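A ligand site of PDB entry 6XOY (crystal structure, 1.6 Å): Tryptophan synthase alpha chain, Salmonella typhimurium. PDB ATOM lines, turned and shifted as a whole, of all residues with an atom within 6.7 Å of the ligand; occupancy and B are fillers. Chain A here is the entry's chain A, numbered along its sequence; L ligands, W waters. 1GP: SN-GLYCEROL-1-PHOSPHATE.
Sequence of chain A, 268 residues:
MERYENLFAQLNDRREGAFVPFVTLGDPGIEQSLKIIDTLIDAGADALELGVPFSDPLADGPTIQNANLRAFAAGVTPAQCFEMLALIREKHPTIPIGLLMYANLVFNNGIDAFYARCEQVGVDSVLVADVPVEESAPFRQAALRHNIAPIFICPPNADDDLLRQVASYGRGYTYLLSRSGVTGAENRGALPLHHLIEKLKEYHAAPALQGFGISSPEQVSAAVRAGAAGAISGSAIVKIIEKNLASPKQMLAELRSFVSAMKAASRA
Water W4 lies within hydrogen-bond range of the backbone NH (N) of Ala 236 (2.5 Å), an oxygen (O3P) of the ligand (2.8 Å), the backbone carbonyl oxygen (O) of Ile 214 (3.0 Å), the backbone NH (N) of Ser 235 (3.3 Å) and the side-chain hydroxyl (OG) of Ser 233 (3.4 Å). Water W1 lies within hydrogen-bond range of OD1 of Asp 60 and O3 of the ligand.
Merely in contact with the ligand: Phe 22 (3.7 Å), Ile 64 (3.1 Å), Leu 100 (3.1 Å), Thr 183 (3.5 Å), Phe 212 (3.4 Å) and Ser 233 (3.9 Å). Hydrophobic or aromatic side chains that line the ligand: Phe 22, Ile 64, Leu 100, Tyr 175 and Phe 212. Of the 27 residues printed, 11 come within 4 Å of the ligand. The nearest printed residue that does not touch the ligand is Ile 232 (4.05 Å).
The backbone NH (N) of Gly 184 lies close to the side-chain hydroxyl (OG) of Ser 235. NH2 of Arg 179 is in hydrogen-bond range of O of Gly 184 (3.3 Å). OD1 of Asp 60 lies within hydrogen-bond range of OG1 of Thr 183 (2.9 Å). The backbone carbonyl oxygen of Ser 233 lies within hydrogen-bond range of the backbone NH of Phe 22, at 2.8 Å. O of Ile 214 lies within hydrogen-bond range of OG of Ser 233 (2.9 Å).
An oxygen (O4P) of the ligand lies within hydrogen-bond range of the backbone NH (N) of Ser 235 (2.7 Å). An oxygen (O4P) of the ligand sits at hydrogen-bond distance from the side-chain hydroxyl of Ser 235, at 2.6 Å. O2 of the ligand is in hydrogen-bond range of OH of Tyr 175 (2.6 Å). An oxygen (O2P) of the ligand sits at hydrogen-bond distance from the backbone NH (N) of Gly 184. An oxygen (O2P) of the ligand is in hydrogen-bond range of the backbone NH of Gly 213, 2.8 Å away. N of Gly 234 sits at hydrogen-bond distance from O3P of the ligand (2.9 Å).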
ATOM      1  N   PHE A  22     -23.077   0.192  15.855  1.00  0.00           N
ATOM      2  CA  PHE A  22     -24.340  -0.342  15.347  1.00  0.00           C
ATOM      3  C   PHE A  22     -24.094  -1.016  14.007  1.00  0.00           C
ATOM      4  O   PHE A  22     -23.412  -0.470  13.122  1.00  0.00           O
ATOM      5  CB  PHE A  22     -25.395   0.742  15.239  1.00  0.00           C
ATOM      6  CG  PHE A  22     -26.569   0.370  14.343  1.00  0.00           C
ATOM      7  CD1 PHE A  22     -26.462   0.437  12.974  1.00  0.00           C
ATOM      8  CD2 PHE A  22     -27.755  -0.083  14.896  1.00  0.00           C
ATOM      9  CE1 PHE A  22     -27.554   0.067  12.128  1.00  0.00           C
ATOM     10  CE2 PHE A  22     -28.833  -0.449  14.103  1.00  0.00           C
ATOM     11  CZ  PHE A  22     -28.739  -0.383  12.719  1.00  0.00           C
ATOM     12  N   GLU A  49     -25.247  -2.201  19.500  1.00  0.00           N
ATOM     13  CA  GLU A  49     -26.585  -1.839  19.039  1.00  0.00           C
ATOM     14  C   GLU A  49     -26.830  -2.574  17.733  1.00  0.00           C
ATOM     15  O   GLU A  49     -25.970  -2.569  16.840  1.00  0.00           O
ATOM     16  CB  GLU A  49     -26.732  -0.343  18.859  1.00  0.00           C
ATOM     17  CG  GLU A  49     -26.788   0.438  20.163  1.00  0.00           C
ATOM     18  CD  GLU A  49     -27.900  -0.060  21.100  1.00  0.00           C
ATOM     19  OE1 GLU A  49     -29.014  -0.349  20.602  1.00  0.00           O
ATOM     20  OE2 GLU A  49     -27.646  -0.189  22.319  1.00  0.00           O
ATOM     21  N   ASP A  60     -33.652   6.226   8.990  1.00  0.00           N
ATOM     22  CA  ASP A  60     -32.361   5.898   8.420  1.00  0.00           C
ATOM     23  C   ASP A  60     -32.155   6.527   7.063  1.00  0.00           C
ATOM     24  O   ASP A  60     -33.066   6.550   6.227  1.00  0.00           O
ATOM     25  CB  ASP A  60     -32.201   4.364   8.294  1.00  0.00           C
ATOM     26  CG  ASP A  60     -32.018   3.692   9.633  1.00  0.00           C
ATOM     27  OD1 ASP A  60     -31.107   4.130  10.388  1.00  0.00           O
ATOM     28  OD2 ASP A  60     -32.784   2.734   9.935  1.00  0.00           O
ATOM     29  N   THR A  63     -27.226   4.936   3.727  1.00  0.00           N
ATOM     30  CA  THR A  63     -26.281   3.880   4.080  1.00  0.00           C
ATOM     31  C   THR A  63     -26.978   2.731   4.797  1.00  0.00           C
ATOM     32  O   THR A  63     -26.778   1.567   4.462  1.00  0.00           O
ATOM     33  CB  THR A  63     -25.156   4.446   4.960  1.00  0.00           C
ATOM     34  OG1 THR A  63     -24.388   5.390   4.203  1.00  0.00           O
ATOM     35  CG2 THR A  63     -24.231   3.312   5.414  1.00  0.00           C
ATOM     36  N   ILE A  64     -27.822   3.043   5.779  1.00  0.00           N
ATOM     37  CA  ILE A  64     -28.466   1.945   6.500  1.00  0.00           C
ATOM     38  C   ILE A  64     -29.687   1.438   5.760  1.00  0.00           C
ATOM     39  O   ILE A  64     -30.009   0.249   5.858  1.00  0.00           O
ATOM     40  CB  ILE A  64     -28.760   2.363   7.954  1.00  0.00           C
ATOM     41  CG1 ILE A  64     -27.390   2.421   8.715  1.00  0.00           C
ATOM     42  CG2 ILE A  64     -29.717   1.366   8.626  1.00  0.00           C
ATOM     43  CD1 ILE A  64     -27.447   3.090  10.082  1.00  0.00           C
ATOM     44  N   LEU A 100     -32.276  -1.898  18.104  1.00  0.00           N
ATOM     45  CA  LEU A 100     -32.908  -0.697  17.558  1.00  0.00           C
ATOM     46  C   LEU A 100     -34.004  -1.227  16.626  1.00  0.00           C
ATOM     47  O   LEU A 100     -33.711  -1.840  15.592  1.00  0.00           O
ATOM     48  CB  LEU A 100     -31.932   0.191  16.803  1.00  0.00           C
ATOM     49  CG  LEU A 100     -30.716   0.809  17.473  1.00  0.00           C
ATOM     50  CD1 LEU A 100     -30.094   1.869  16.552  1.00  0.00           C
ATOM     51  CD2 LEU A 100     -31.061   1.423  18.796  1.00  0.00           C
ATOM     52  N   LEU A 127     -34.695  -0.119  21.936  1.00  0.00           N
ATOM     53  CA  LEU A 127     -35.143   1.211  21.513  1.00  0.00           C
ATOM     54  C   LEU A 127     -36.095   1.014  20.354  1.00  0.00           C
ATOM     55  O   LEU A 127     -35.784   0.308  19.391  1.00  0.00           O
ATOM     56  CB  LEU A 127     -33.936   2.095  21.139  1.00  0.00           C
ATOM     57  CG  LEU A 127     -34.198   3.560  20.744  1.00  0.00           C
ATOM     58  CD1 LEU A 127     -32.911   4.417  20.801  1.00  0.00           C
ATOM     59  CD2 LEU A 127     -34.821   3.657  19.352  1.00  0.00           C
ATOM     60  N   TYR A 175     -30.448   7.638  25.021  1.00  0.00           N
ATOM     61  CA  TYR A 175     -29.937   7.881  23.680  1.00  0.00           C
ATOM     62  C   TYR A 175     -29.987   9.377  23.420  1.00  0.00           C
ATOM     63  O   TYR A 175     -31.045   9.981  23.369  1.00  0.00           O
ATOM     64  CB  TYR A 175     -30.709   7.099  22.631  1.00  0.00           C
ATOM     65  CG  TYR A 175     -30.026   7.037  21.266  1.00  0.00           C
ATOM     66  CD1 TYR A 175     -29.778   8.191  20.504  1.00  0.00           C
ATOM     67  CD2 TYR A 175     -29.664   5.818  20.724  1.00  0.00           C
ATOM     68  CE1 TYR A 175     -29.164   8.102  19.262  1.00  0.00           C
ATOM     69  CE2 TYR A 175     -29.063   5.712  19.482  1.00  0.00           C
ATOM     70  CZ  TYR A 175     -28.806   6.863  18.751  1.00  0.00           C
ATOM     71  OH  TYR A 175     -28.205   6.740  17.524  1.00  0.00           O
ATOM     72  N   ARG A 179     -28.297  15.513  16.550  1.00  0.00           N
ATOM     73  CA  ARG A 179     -28.840  16.482  15.599  1.00  0.00           C
ATOM     74  C   ARG A 179     -30.187  15.947  15.096  1.00  0.00           C
ATOM     75  O   ARG A 179     -30.558  14.806  15.348  1.00  0.00           O
ATOM     76  CB  ARG A 179     -27.891  16.697  14.406  1.00  0.00           C
ATOM     77  CG  ARG A 179     -27.526  15.352  13.755  1.00  0.00           C
ATOM     78  CD  ARG A 179     -27.136  15.500  12.288  1.00  0.00           C
ATOM     79  NE  ARG A 179     -26.712  14.203  11.728  1.00  0.00           N
ATOM     80  CZ  ARG A 179     -27.545  13.275  11.276  1.00  0.00           C
ATOM     81  NH1 ARG A 179     -28.858  13.419  11.347  1.00  0.00           N
ATOM     82  NH2 ARG A 179     -27.034  12.169  10.731  1.00  0.00           N
ATOM     83  N   VAL A 182     -31.962  12.136   9.736  1.00  0.00           N
ATOM     84  CA  VAL A 182     -31.870  10.695   9.774  1.00  0.00           C
ATOM     85  C   VAL A 182     -30.406  10.291   9.913  1.00  0.00           C
ATOM     86  O   VAL A 182     -29.488  11.095   9.798  1.00  0.00           O
ATOM     87  CB  VAL A 182     -32.509  10.016   8.542  1.00  0.00           C
ATOM     88  CG1 VAL A 182     -33.996  10.250   8.528  1.00  0.00           C
ATOM     89  CG2 VAL A 182     -31.863  10.519   7.235  1.00  0.00           C
ATOM     90  N   THR A 183     -30.197   9.002  10.154  1.00  0.00           N
ATOM     91  CA  THR A 183     -28.852   8.496  10.322  1.00  0.00           C
ATOM     92  C   THR A 183     -28.008   8.820   9.101  1.00  0.00           C
ATOM     93  O   THR A 183     -28.526   9.004   7.992  1.00  0.00           O
ATOM     94  CB  THR A 183     -28.872   6.991  10.576  1.00  0.00           C
ATOM     95  OG1 THR A 183     -29.357   6.297   9.426  1.00  0.00           O
ATOM     96  CG2 THR A 183     -29.756   6.668  11.764  1.00  0.00           C
ATOM     97  N   GLY A 184     -26.703   8.910   9.315  1.00  0.00           N
ATOM     98  CA  GLY A 184     -25.784   9.083   8.215  1.00  0.00           C
ATOM     99  C   GLY A 184     -24.462   9.631   8.673  1.00  0.00           C
ATOM    100  O   GLY A 184     -24.419  10.596   9.450  1.00  0.00           O
ATOM    101  N   ALA A 185     -23.363   9.043   8.181  1.00  0.00           N
ATOM    102  CA  ALA A 185     -22.044   9.496   8.572  1.00  0.00           C
ATOM    103  C   ALA A 185     -21.662  10.820   7.905  1.00  0.00           C
ATOM    104  O   ALA A 185     -20.829  11.554   8.439  1.00  0.00           O
ATOM    105  CB  ALA A 185     -21.011   8.421   8.230  1.00  0.00           C
ATOM    106  N   GLU A 186     -22.285  11.135   6.766  1.00  0.00           N
ATOM    107  CA  GLU A 186     -21.911  12.341   6.026  1.00  0.00           C
ATOM    108  C   GLU A 186     -22.299  13.600   6.781  1.00  0.00           C
ATOM    109  O   GLU A 186     -21.667  14.643   6.621  1.00  0.00           O
ATOM    110  CB  GLU A 186     -22.556  12.322   4.636  1.00  0.00           C
ATOM    111  CG  GLU A 186     -22.408  10.999   3.889  1.00  0.00           C
ATOM    112  CD  GLU A 186     -23.600  10.049   4.061  1.00  0.00           C
ATOM    113  OE1 GLU A 186     -24.478  10.301   4.921  1.00  0.00           O
ATOM    114  OE2 GLU A 186     -23.666   9.046   3.307  1.00  0.00           O
ATOM    115  N   ASN A 187     -23.326  13.535   7.623  1.00  0.00           N
ATOM    116  CA  ASN A 187     -23.887  14.688   8.322  1.00  0.00           C
ATOM    117  C   ASN A 187     -23.457  14.634   9.779  1.00  0.00           C
ATOM    118  O   ASN A 187     -23.933  13.789  10.547  1.00  0.00           O
ATOM    119  CB  ASN A 187     -25.407  14.702   8.186  1.00  0.00           C
ATOM    120  CG  ASN A 187     -26.069  15.780   9.028  1.00  0.00           C
ATOM    121  OD1 ASN A 187     -25.403  16.666   9.582  1.00  0.00           O
ATOM    122  ND2 ASN A 187     -27.413  15.698   9.132  1.00  0.00           N
ATOM    123  N   GLY A 211     -25.549   9.613  19.717  1.00  0.00           N
ATOM    124  CA  GLY A 211     -25.558   9.001  18.400  1.00  0.00           C
ATOM    125  C   GLY A 211     -26.128   9.905  17.322  1.00  0.00           C
ATOM    126  O   GLY A 211     -26.830  10.876  17.608  1.00  0.00           O
ATOM    127  N   PHE A 212     -25.875   9.488  16.057  1.00  0.00           N
ATOM    128  CA  PHE A 212     -26.160  10.110  14.781  1.00  0.00           C
ATOM    129  C   PHE A 212     -24.946  10.889  14.268  1.00  0.00           C
ATOM    130  O   PHE A 212     -24.478  11.810  14.944  1.00  0.00           O
ATOM    131  CB  PHE A 212     -27.348  11.076  14.793  1.00  0.00           C
ATOM    132  CG  PHE A 212     -28.685  10.381  14.581  1.00  0.00           C
ATOM    133  CD1 PHE A 212     -28.924   9.151  15.162  1.00  0.00           C
ATOM    134  CD2 PHE A 212     -29.672  10.959  13.799  1.00  0.00           C
ATOM    135  CE1 PHE A 212     -30.148   8.507  14.956  1.00  0.00           C
ATOM    136  CE2 PHE A 212     -30.884  10.316  13.609  1.00  0.00           C
ATOM    137  CZ  PHE A 212     -31.124   9.108  14.187  1.00  0.00           C
ATOM    138  N   GLY A 213     -24.459  10.556  13.063  1.00  0.00           N
ATOM    139  CA  GLY A 213     -23.384  11.312  12.445  1.00  0.00           C
ATOM    140  C   GLY A 213     -22.031  11.284  13.149  1.00  0.00           C
ATOM    141  O   GLY A 213     -21.240  12.214  12.999  1.00  0.00           O
ATOM    142  N   ILE A 214     -21.765  10.256  13.944  1.00  0.00           N
ATOM    143  CA  ILE A 214     -20.465  10.107  14.612  1.00  0.00           C
ATOM    144  C   ILE A 214     -19.668   9.113  13.794  1.00  0.00           C
ATOM    145  O   ILE A 214     -20.038   7.938  13.684  1.00  0.00           O
ATOM    146  CB  ILE A 214     -20.624   9.661  16.070  1.00  0.00           C
ATOM    147  CG1 ILE A 214     -21.022  10.874  16.929  1.00  0.00           C
ATOM    148  CG2 ILE A 214     -19.311   9.057  16.587  1.00  0.00           C
ATOM    149  CD1 ILE A 214     -21.412  10.532  18.310  1.00  0.00           C
ATOM    150  N   SER A 215     -18.567   9.585  13.206  1.00  0.00           N
ATOM    151  CA  SER A 215     -17.836   8.792  12.231  1.00  0.00           C
ATOM    152  C   SER A 215     -16.331   8.973  12.323  1.00  0.00           C
ATOM    153  O   SER A 215     -15.609   8.441  11.474  1.00  0.00           O
ATOM    154  CB  SER A 215     -18.297   9.122  10.801  1.00  0.00           C
ATOM    155  OG  SER A 215     -18.084  10.495  10.490  1.00  0.00           O
ATOM    156  N   ILE A 232     -22.268   6.137  19.966  1.00  0.00           N
ATOM    157  CA  ILE A 232     -22.721   5.120  19.039  1.00  0.00           C
ATOM    158  C   ILE A 232     -22.327   5.555  17.634  1.00  0.00           C
ATOM    159  O   ILE A 232     -22.436   6.737  17.282  1.00  0.00           O
ATOM    160  CB  ILE A 232     -24.261   4.947  19.157  1.00  0.00           C
ATOM    161  CG1 ILE A 232     -24.634   4.551  20.592  1.00  0.00           C
ATOM    162  CG2 ILE A 232     -24.788   3.959  18.145  1.00  0.00           C
ATOM    163  CD1 ILE A 232     -26.073   4.882  20.947  1.00  0.00           C
ATOM    164  N   SER A 233     -21.888   4.592  16.810  1.00  0.00           N
ATOM    165  CA  SER A 233     -21.601   4.846  15.393  1.00  0.00           C
ATOM    166  C   SER A 233     -22.156   3.701  14.562  1.00  0.00           C
ATOM    167  O   SER A 233     -21.846   2.526  14.813  1.00  0.00           O
ATOM    168  CB  SER A 233     -20.107   5.011  15.184  1.00  0.00           C
ATOM    169  OG  SER A 233     -19.760   5.103  13.823  1.00  0.00           O
ATOM    170  N   GLY A 234     -23.022   4.027  13.585  1.00  0.00           N
ATOM    171  CA  GLY A 234     -23.612   3.023  12.730  1.00  0.00           C
ATOM    172  C   GLY A 234     -23.222   3.176  11.276  1.00  0.00           C
ATOM    173  O   GLY A 234     -22.534   2.318  10.719  1.00  0.00           O
ATOM    174  N   SER A 235     -23.662   4.270  10.646  1.00  0.00           N
ATOM    175  CA  SER A 235     -23.388   4.455   9.219  1.00  0.00           C
ATOM    176  C   SER A 235     -21.899   4.352   8.908  1.00  0.00           C
ATOM    177  O   SER A 235     -21.494   3.734   7.913  1.00  0.00           O
ATOM    178  CB  SER A 235     -23.935   5.808   8.759  1.00  0.00           C
ATOM    179  OG  SER A 235     -25.345   5.780   8.821  1.00  0.00           O
ATOM    180  N   ALA A 236     -21.070   4.973   9.728  1.00  0.00           N
ATOM    181  CA  ALA A 236     -19.625   4.893   9.490  1.00  0.00           C
ATOM    182  C   ALA A 236     -19.152   3.440   9.436  1.00  0.00           C
ATOM    183  O   ALA A 236     -18.303   3.082   8.597  1.00  0.00           O
ATOM    184  CB  ALA A 236     -18.878   5.648  10.587  1.00  0.00           C
ATOM    185  N   ILE A 237     -19.686   2.594  10.316  1.00  0.00           N
ATOM    186  CA  ILE A 237     -19.303   1.193  10.306  1.00  0.00           C
ATOM    187  C   ILE A 237     -19.930   0.465   9.133  1.00  0.00           C
ATOM    188  O   ILE A 237     -19.271  -0.341   8.452  1.00  0.00           O
ATOM    189  CB  ILE A 237     -19.684   0.547  11.654  1.00  0.00           C
ATOM    190  CG1 ILE A 237     -18.672   0.957  12.718  1.00  0.00           C
ATOM    191  CG2 ILE A 237     -19.754  -0.963  11.507  1.00  0.00           C
ATOM    192  CD1 ILE A 237     -19.303   1.281  14.043  1.00  0.00           C
ATOM    193  N   VAL A 238     -21.211   0.735   8.867  1.00  0.00           N
ATOM    194  CA  VAL A 238     -21.884   0.099   7.738  1.00  0.00           C
ATOM    195  C   VAL A 238     -21.213   0.486   6.421  1.00  0.00           C
ATOM    196  O   VAL A 238     -21.105  -0.340   5.507  1.00  0.00           O
ATOM    197  CB  VAL A 238     -23.388   0.466   7.752  1.00  0.00           C
ATOM    198  CG1 VAL A 238     -24.105  -0.080   6.521  1.00  0.00           C
ATOM    199  CG2 VAL A 238     -24.059  -0.057   9.043  1.00  0.00           C
HETATM  200  C3  1GP L   1     -27.685   3.791  15.301  1.00  0.00           C
HETATM  201  O3  1GP L   1     -27.092   4.149  13.023  1.00  0.00           O
HETATM  202  C2  1GP L   1     -27.429   4.850  14.202  1.00  0.00           C
HETATM  203  O2  1GP L   1     -28.376   4.432  16.335  1.00  0.00           O
HETATM  204  C1  1GP L   1     -26.372   5.858  14.553  1.00  0.00           C
HETATM  205  O1P 1GP L   1     -26.403   6.926  13.599  1.00  0.00           O
HETATM  206  O2P 1GP L   1     -25.459   8.315  11.708  1.00  0.00           O
HETATM  207  O3P 1GP L   1     -23.984   6.727  12.918  1.00  0.00           O
HETATM  208  O4P 1GP L   1     -25.662   5.886  11.376  1.00  0.00           O
HETATM  209  P   1GP L   1     -25.406   6.937  12.371  1.00  0.00           P
HETATM  210  O   HOH W   1     -30.088   3.230  13.084  1.00  0.00           O
HETATM  211  O   HOH W   2     -23.605   7.948  15.123  1.00  0.00           O
HETATM  212  O   HOH W   3     -31.266   4.817  15.309  1.00  0.00           O
HETATM  213  O   HOH W   4     -21.587   6.698  11.394  1.00  0.00           O
